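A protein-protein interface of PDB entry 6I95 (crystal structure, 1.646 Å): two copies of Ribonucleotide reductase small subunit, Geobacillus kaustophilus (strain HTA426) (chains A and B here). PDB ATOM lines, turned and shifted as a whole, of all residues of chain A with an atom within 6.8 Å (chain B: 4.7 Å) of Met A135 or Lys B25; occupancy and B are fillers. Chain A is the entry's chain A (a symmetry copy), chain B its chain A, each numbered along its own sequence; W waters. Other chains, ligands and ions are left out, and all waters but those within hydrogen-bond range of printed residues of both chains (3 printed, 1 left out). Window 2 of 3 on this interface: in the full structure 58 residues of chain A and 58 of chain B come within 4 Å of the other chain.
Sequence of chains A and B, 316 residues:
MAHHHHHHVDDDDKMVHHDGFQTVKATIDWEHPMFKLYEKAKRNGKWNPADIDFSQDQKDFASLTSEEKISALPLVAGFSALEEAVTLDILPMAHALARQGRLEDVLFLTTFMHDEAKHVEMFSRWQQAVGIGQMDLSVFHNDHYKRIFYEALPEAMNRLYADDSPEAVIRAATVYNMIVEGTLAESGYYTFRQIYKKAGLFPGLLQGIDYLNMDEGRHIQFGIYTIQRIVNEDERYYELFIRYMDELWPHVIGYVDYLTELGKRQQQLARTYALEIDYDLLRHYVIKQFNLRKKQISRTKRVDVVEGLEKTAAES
Water W3 lies within hydrogen-bond range of the side-chain hydroxyl (OG) of Ser A138 and the backbone NH (N) of Phe B21. Water W2 lies within hydrogen-bond range of O of Ala B26, O of Thr B23 and NE2 of Gln A127. Water W1 lies within hydrogen-bond range of the backbone carbonyl oxygen (O) of Lys B25 and the backbone carbonyl oxygen (O) of Gln A134.
No position is printed for both chains. Of the 12 pairs that touch across the chains among the printed residues, none has its exchanged pair printed and touching as well.
N of Gln B22 lies within hydrogen-bond range of OE2 of Glu A84. The side-chain hydroxyl of Thr B23 is in hydrogen-bond range of the side-chain carboxylate of Glu A84 (2.7 Å). The backbone carbonyl oxygen (O) of Thr B23 lies within hydrogen-bond range of the side-chain amide nitrogen (NE2) of Gln A127 (3.0 Å). The backbone carbonyl oxygen (O) of Met A135 sits close to the backbone carbonyl oxygen (O) of Val B24, at 3.4 Å. The backbone carbonyl oxygen (O) of Gly A133 sits close to the backbone carbonyl oxygen (O) of Ala B26 (3.4 Å). The backbone carbonyl oxygen (O) of Val B24 lies within hydrogen-bond range of the backbone NH (N) of Leu A137, at 2.9 Å.
Of the printed residues of chain B, Gln A127 touches Thr B23 (3.0 Å). Met A135 touches just these residues of chain B: Val B24 and Lys B25. Val A139 touches none of the printed residues of chain B. Of the printed residues of chain A, Thr B23 touches Glu A84 and Gln A127. Printed residues of chain A within 4 Å of Lys B25: Met A135 (3.7 Å), Asp A136 (3.6 Å) and Ser A138 (3.8 Å). Of the printed residues of chain A, Ala B26 touches Gly A133. The nearest residue of chain A that does not touch Lys B25 is Gly A133 (4.2 Å).
Among the printed residues, pairs that only touch across the chains: Ser A138 with Val B24, Glu A84 with Phe B21, Asp A136 with Lys B25, Met A135 with Lys B25, Asp A136 with Val B24 and Ser A138 with Lys B25.
Hydrophobic or aromatic side chains of chain A within 4 Å of the printed part of chain B: Leu A137. Along chain A the printed residues that touch a printed residue of chain B span positions 84 to 138. Of the 8 printed residues of chain B, 6 touch a printed residue of chain A. Among the printed residues, 12 pairs touch across the chains. Among the printed residues, no Asp or Glu carboxylate lies within 4 Å of a Lys or Arg side-chain nitrogen of the other chain.
The backbone carbonyl oxygen of Gln A127 is in hydrogen-bond range of the backbone NH of Gly A133 (3.3 Å). The backbone carbonyl oxygen of Gln A127 is in hydrogen-bond range of the backbone NH of Ile A132 (3.1 Å). The side-chain hydroxyl (OG) of Ser A138 sits at hydrogen-bond distance from the side-chain carboxylate (OD1) of Asp A136 (3.0 Å).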
ATOM      1  N   PHE A  61       7.938 -16.222   5.030  1.00  0.00           N
ATOM      2  CA  PHE A  61       9.183 -15.722   5.581  1.00  0.00           C
ATOM      3  C   PHE A  61      10.171 -15.426   4.455  1.00  0.00           C
ATOM      4  O   PHE A  61      10.893 -14.432   4.514  1.00  0.00           O
ATOM      5  CB  PHE A  61       9.790 -16.755   6.550  1.00  0.00           C
ATOM      6  CG  PHE A  61      10.869 -16.206   7.449  1.00  0.00           C
ATOM      7  CD1 PHE A  61      10.552 -15.482   8.578  1.00  0.00           C
ATOM      8  CD2 PHE A  61      12.197 -16.463   7.196  1.00  0.00           C
ATOM      9  CE1 PHE A  61      11.531 -14.985   9.422  1.00  0.00           C
ATOM     10  CE2 PHE A  61      13.182 -15.954   8.042  1.00  0.00           C
ATOM     11  CZ  PHE A  61      12.832 -15.227   9.161  1.00  0.00           C
ATOM     12  N   ILE A  70      14.120  -9.901  10.254  1.00  0.00           N
ATOM     13  CA  ILE A  70      14.640  -9.835  11.621  1.00  0.00           C
ATOM     14  C   ILE A  70      13.683  -9.137  12.564  1.00  0.00           C
ATOM     15  O   ILE A  70      13.854  -9.241  13.783  1.00  0.00           O
ATOM     16  CB  ILE A  70      16.015  -9.144  11.760  1.00  0.00           C
ATOM     17  CG1 ILE A  70      15.929  -7.611  11.662  1.00  0.00           C
ATOM     18  CG2 ILE A  70      16.992  -9.717  10.740  1.00  0.00           C
ATOM     19  CD1 ILE A  70      17.171  -6.930  12.203  1.00  0.00           C
ATOM     20  N   LEU A  73      12.170 -11.844  14.671  1.00  0.00           N
ATOM     21  CA  LEU A  73      13.004 -12.804  15.390  1.00  0.00           C
ATOM     22  C   LEU A  73      13.107 -12.542  16.893  1.00  0.00           C
ATOM     23  O   LEU A  73      13.221 -13.507  17.657  1.00  0.00           O
ATOM     24  CB  LEU A  73      14.414 -12.845  14.792  1.00  0.00           C
ATOM     25  CG  LEU A  73      14.488 -13.250  13.313  1.00  0.00           C
ATOM     26  CD1 LEU A  73      15.922 -13.242  12.868  1.00  0.00           C
ATOM     27  CD2 LEU A  73      13.882 -14.606  13.055  1.00  0.00           C
ATOM     28  N   GLU A  84      11.184 -23.490  26.560  1.00  0.00           N
ATOM     29  CA  GLU A  84      12.171 -24.458  27.009  1.00  0.00           C
ATOM     30  C   GLU A  84      12.411 -24.329  28.505  1.00  0.00           C
ATOM     31  O   GLU A  84      12.414 -25.340  29.220  1.00  0.00           O
ATOM     32  CB  GLU A  84      13.474 -24.292  26.222  1.00  0.00           C
ATOM     33  CG  GLU A  84      14.502 -25.370  26.487  1.00  0.00           C
ATOM     34  CD  GLU A  84      15.666 -25.284  25.492  1.00  0.00           C
ATOM     35  OE1 GLU A  84      15.445 -24.878  24.317  1.00  0.00           O
ATOM     36  OE2 GLU A  84      16.798 -25.623  25.880  1.00  0.00           O
ATOM     37  N   GLN A 127      10.889 -22.607  13.459  1.00  0.00           N
ATOM     38  CA  GLN A 127      12.209 -22.090  13.088  1.00  0.00           C
ATOM     39  C   GLN A 127      12.844 -22.960  11.996  1.00  0.00           C
ATOM     40  O   GLN A 127      13.399 -22.457  11.004  1.00  0.00           O
ATOM     41  CB  GLN A 127      13.115 -22.032  14.324  1.00  0.00           C
ATOM     42  CG  GLN A 127      12.746 -20.990  15.380  1.00  0.00           C
ATOM     43  CD  GLN A 127      13.856 -20.835  16.392  1.00  0.00           C
ATOM     44  OE1 GLN A 127      15.035 -20.817  16.023  1.00  0.00           O
ATOM     45  NE2 GLN A 127      13.503 -20.757  17.664  1.00  0.00           N
ATOM     46  N   GLY A 131      13.620 -21.665   7.967  1.00  0.00           N
ATOM     47  CA  GLY A 131      15.021 -21.559   7.602  1.00  0.00           C
ATOM     48  C   GLY A 131      15.911 -20.771   8.531  1.00  0.00           C
ATOM     49  O   GLY A 131      16.971 -20.317   8.081  1.00  0.00           O
ATOM     50  N   ILE A 132      15.548 -20.606   9.810  1.00  0.00           N
ATOM     51  CA  ILE A 132      16.371 -19.910  10.785  1.00  0.00           C
ATOM     52  C   ILE A 132      16.845 -20.817  11.910  1.00  0.00           C
ATOM     53  O   ILE A 132      17.402 -20.328  12.875  1.00  0.00           O
ATOM     54  CB  ILE A 132      15.652 -18.679  11.374  1.00  0.00           C
ATOM     55  CG1 ILE A 132      14.421 -19.082  12.185  1.00  0.00           C
ATOM     56  CG2 ILE A 132      15.318 -17.684  10.279  1.00  0.00           C
ATOM     57  CD1 ILE A 132      13.798 -17.911  12.936  1.00  0.00           C
ATOM     58  N   GLY A 133      16.605 -22.122  11.820  1.00  0.00           N
ATOM     59  CA  GLY A 133      17.061 -23.026  12.863  1.00  0.00           C
ATOM     60  C   GLY A 133      18.554 -22.965  13.121  1.00  0.00           C
ATOM     61  O   GLY A 133      18.995 -23.152  14.260  1.00  0.00           O
ATOM     62  N   GLN A 134      19.356 -22.695  12.074  1.00  0.00           N
ATOM     63  CA  GLN A 134      20.800 -22.566  12.222  1.00  0.00           C
ATOM     64  C   GLN A 134      21.241 -21.218  12.807  1.00  0.00           C
ATOM     65  O   GLN A 134      22.411 -21.074  13.161  1.00  0.00           O
ATOM     66  CB  GLN A 134      21.484 -22.804  10.858  1.00  0.00           C
ATOM     67  CG  GLN A 134      21.365 -21.694   9.831  1.00  0.00           C
ATOM     68  CD  GLN A 134      19.978 -21.450   9.291  1.00  0.00           C
ATOM     69  OE1 GLN A 134      19.082 -22.302   9.373  1.00  0.00           O
ATOM     70  NE2 GLN A 134      19.790 -20.265   8.697  1.00  0.00           N
ATOM     71  N   MET A 135      20.348 -20.240  12.946  1.00  0.00           N
ATOM     72  CA  MET A 135      20.696 -18.942  13.499  1.00  0.00           C
ATOM     73  C   MET A 135      20.644 -18.954  15.024  1.00  0.00           C
ATOM     74  O   MET A 135      19.682 -19.431  15.616  1.00  0.00           O
ATOM     75  CB  MET A 135      19.738 -17.903  12.938  1.00  0.00           C
ATOM     76  CG  MET A 135      20.103 -16.467  13.201  1.00  0.00           C
ATOM     77  SD  MET A 135      18.814 -15.393  12.523  1.00  0.00           S
ATOM     78  CE  MET A 135      18.444 -16.227  10.989  1.00  0.00           C
ATOM     79  N   ASP A 136      21.681 -18.422  15.667  1.00  0.00           N
ATOM     80  CA  ASP A 136      21.691 -18.335  17.123  1.00  0.00           C
ATOM     81  C   ASP A 136      20.929 -17.080  17.534  1.00  0.00           C
ATOM     82  O   ASP A 136      21.415 -15.953  17.368  1.00  0.00           O
ATOM     83  CB  ASP A 136      23.119 -18.317  17.663  1.00  0.00           C
ATOM     84  CG  ASP A 136      23.175 -18.322  19.184  1.00  0.00           C
ATOM     85  OD1 ASP A 136      22.141 -18.102  19.853  1.00  0.00           O
ATOM     86  OD2 ASP A 136      24.273 -18.543  19.729  1.00  0.00           O
ATOM     87  N   LEU A 137      19.714 -17.266  18.044  1.00  0.00           N
ATOM     88  CA  LEU A 137      18.841 -16.150  18.372  1.00  0.00           C
ATOM     89  C   LEU A 137      19.089 -15.573  19.779  1.00  0.00           C
ATOM     90  O   LEU A 137      18.360 -14.678  20.204  1.00  0.00           O
ATOM     91  CB  LEU A 137      17.375 -16.600  18.203  1.00  0.00           C
ATOM     92  CG  LEU A 137      16.938 -17.050  16.805  1.00  0.00           C
ATOM     93  CD1 LEU A 137      15.423 -17.303  16.793  1.00  0.00           C
ATOM     94  CD2 LEU A 137      17.316 -16.033  15.739  1.00  0.00           C
ATOM     95  N   SER A 138      20.111 -16.041  20.501  1.00  0.00           N
ATOM     96  CA  SER A 138      20.387 -15.556  21.854  1.00  0.00           C
ATOM     97  C   SER A 138      20.735 -14.080  21.901  1.00  0.00           C
ATOM     98  O   SER A 138      20.662 -13.470  22.978  1.00  0.00           O
ATOM     99  CB  SER A 138      21.560 -16.335  22.463  1.00  0.00           C
ATOM    100  OG  SER A 138      21.212 -17.702  22.634  1.00  0.00           O
ATOM    101  N   VAL A 139      21.148 -13.510  20.770  1.00  0.00           N
ATOM    102  CA  VAL A 139      21.457 -12.088  20.711  1.00  0.00           C
ATOM    103  C   VAL A 139      20.259 -11.213  21.070  1.00  0.00           C
ATOM    104  O   VAL A 139      20.432 -10.038  21.415  1.00  0.00           O
ATOM    105  CB  VAL A 139      22.005 -11.742  19.304  1.00  0.00           C
ATOM    106  CG1 VAL A 139      21.000 -12.097  18.209  1.00  0.00           C
ATOM    107  CG2 VAL A 139      22.360 -10.272  19.232  1.00  0.00           C
ATOM    108  N   PHE A 140      19.039 -11.748  21.012  1.00  0.00           N
ATOM    109  CA  PHE A 140      17.855 -10.965  21.355  1.00  0.00           C
ATOM    110  C   PHE A 140      17.397 -11.149  22.803  1.00  0.00           C
ATOM    111  O   PHE A 140      16.273 -10.759  23.147  1.00  0.00           O
ATOM    112  CB  PHE A 140      16.715 -11.299  20.397  1.00  0.00           C
ATOM    113  CG  PHE A 140      17.035 -10.980  18.958  1.00  0.00           C
ATOM    114  CD1 PHE A 140      17.222  -9.663  18.552  1.00  0.00           C
ATOM    115  CD2 PHE A 140      17.179 -11.986  18.026  1.00  0.00           C
ATOM    116  CE1 PHE A 140      17.538  -9.367  17.240  1.00  0.00           C
ATOM    117  CE2 PHE A 140      17.498 -11.690  16.712  1.00  0.00           C
ATOM    118  CZ  PHE A 140      17.676 -10.368  16.324  1.00  0.00           C
ATOM    119  N   ASP B  19      22.387 -21.902  31.046  1.00  0.00           N
ATOM    120  CA  ASP B  19      23.496 -21.340  30.275  1.00  0.00           C
ATOM    121  C   ASP B  19      23.002 -20.705  28.984  1.00  0.00           C
ATOM    122  O   ASP B  19      23.365 -19.571  28.654  1.00  0.00           O
ATOM    123  CB  ASP B  19      24.521 -22.436  29.972  1.00  0.00           C
ATOM    124  CG  ASP B  19      25.543 -22.005  28.948  1.00  0.00           C
ATOM    125  OD1 ASP B  19      25.925 -20.816  28.963  1.00  0.00           O
ATOM    126  OD2 ASP B  19      25.962 -22.850  28.123  1.00  0.00           O
ATOM    127  N   GLY B  20      22.219 -21.439  28.228  1.00  0.00           N
ATOM    128  CA  GLY B  20      21.394 -20.880  27.181  1.00  0.00           C
ATOM    129  C   GLY B  20      20.309 -21.881  26.938  1.00  0.00           C
ATOM    130  O   GLY B  20      20.061 -22.745  27.778  1.00  0.00           O
ATOM    131  N   PHE B  21      19.690 -21.809  25.755  1.00  0.00           N
ATOM    132  CA  PHE B  21      18.602 -22.706  25.393  1.00  0.00           C
ATOM    133  C   PHE B  21      18.858 -23.319  24.025  1.00  0.00           C
ATOM    134  O   PHE B  21      19.163 -22.601  23.065  1.00  0.00           O
ATOM    135  CB  PHE B  21      17.292 -21.920  25.436  1.00  0.00           C
ATOM    136  CG  PHE B  21      16.972 -21.436  26.801  1.00  0.00           C
ATOM    137  CD1 PHE B  21      16.451 -22.301  27.710  1.00  0.00           C
ATOM    138  CD2 PHE B  21      17.278 -20.148  27.206  1.00  0.00           C
ATOM    139  CE1 PHE B  21      16.152 -21.889  29.003  1.00  0.00           C
ATOM    140  CE2 PHE B  21      16.977 -19.725  28.515  1.00  0.00           C
ATOM    141  CZ  PHE B  21      16.434 -20.591  29.400  1.00  0.00           C
ATOM    142  N   GLN B  22      18.728 -24.637  23.931  1.00  0.00           N
ATOM    143  CA  GLN B  22      19.046 -25.331  22.686  1.00  0.00           C
ATOM    144  C   GLN B  22      18.142 -24.878  21.544  1.00  0.00           C
ATOM    145  O   GLN B  22      18.580 -24.815  20.390  1.00  0.00           O
ATOM    146  CB  GLN B  22      18.934 -26.841  22.912  1.00  0.00           C
ATOM    147  CG  GLN B  22      19.236 -27.710  21.708  1.00  0.00           C
ATOM    148  CD  GLN B  22      18.967 -29.166  21.975  1.00  0.00           C
ATOM    149  OE1 GLN B  22      19.224 -29.672  23.086  1.00  0.00           O
ATOM    150  NE2 GLN B  22      18.427 -29.865  20.968  1.00  0.00           N
ATOM    151  N   THR B  23      16.866 -24.578  21.823  1.00  0.00           N
ATOM    152  CA  THR B  23      15.992 -24.188  20.713  1.00  0.00           C
ATOM    153  C   THR B  23      16.083 -22.699  20.392  1.00  0.00           C
ATOM    154  O   THR B  23      15.368 -22.224  19.500  1.00  0.00           O
ATOM    155  CB  THR B  23      14.535 -24.547  20.992  1.00  0.00           C
ATOM    156  OG1 THR B  23      14.086 -23.853  22.163  1.00  0.00           O
ATOM    157  CG2 THR B  23      14.410 -26.022  21.188  1.00  0.00           C
ATOM    158  N   VAL B  24      16.960 -21.968  21.063  1.00  0.00           N
ATOM    159  CA  VAL B  24      17.317 -20.613  20.675  1.00  0.00           C
ATOM    160  C   VAL B  24      18.644 -20.589  19.923  1.00  0.00           C
ATOM    161  O   VAL B  24      18.771 -19.927  18.885  1.00  0.00           O
ATOM    162  CB  VAL B  24      17.364 -19.731  21.936  1.00  0.00           C
ATOM    163  CG1 VAL B  24      17.922 -18.370  21.629  1.00  0.00           C
ATOM    164  CG2 VAL B  24      15.955 -19.599  22.527  1.00  0.00           C
ATOM    165  N   LYS B  25      19.616 -21.363  20.423  1.00  0.00           N
ATOM    166  CA  LYS B  25      20.902 -21.498  19.737  1.00  0.00           C
ATOM    167  C   LYS B  25      20.783 -22.303  18.458  1.00  0.00           C
ATOM    168  O   LYS B  25      21.501 -22.035  17.485  1.00  0.00           O
ATOM    169  CB  LYS B  25      21.921 -22.136  20.694  1.00  0.00           C
ATOM    170  CG  LYS B  25      22.180 -21.316  21.956  1.00  0.00           C
ATOM    171  CD  LYS B  25      23.389 -21.844  22.762  1.00  0.00           C
ATOM    172  CE  LYS B  25      23.058 -23.077  23.599  1.00  0.00           C
ATOM    173  NZ  LYS B  25      24.180 -23.465  24.511  1.00  0.00           N
ATOM    174  N   ALA B  26      19.887 -23.275  18.428  1.00  0.00           N
ATOM    175  CA  ALA B  26      19.781 -24.212  17.322  1.00  0.00           C
ATOM    176  C   ALA B  26      18.352 -24.724  17.238  1.00  0.00           C
ATOM    177  O   ALA B  26      17.432 -23.905  17.206  1.00  0.00           O
ATOM    178  CB  ALA B  26      20.794 -25.358  17.483  1.00  0.00           C
HETATM  179  O   HOH W   1      22.775 -23.530  15.409  1.00  0.00           O
HETATM  180  O   HOH W   2      14.634 -23.993  17.352  1.00  0.00           O
HETATM  181  O   HOH W   3      20.057 -19.100  24.592  1.00  0.00           O
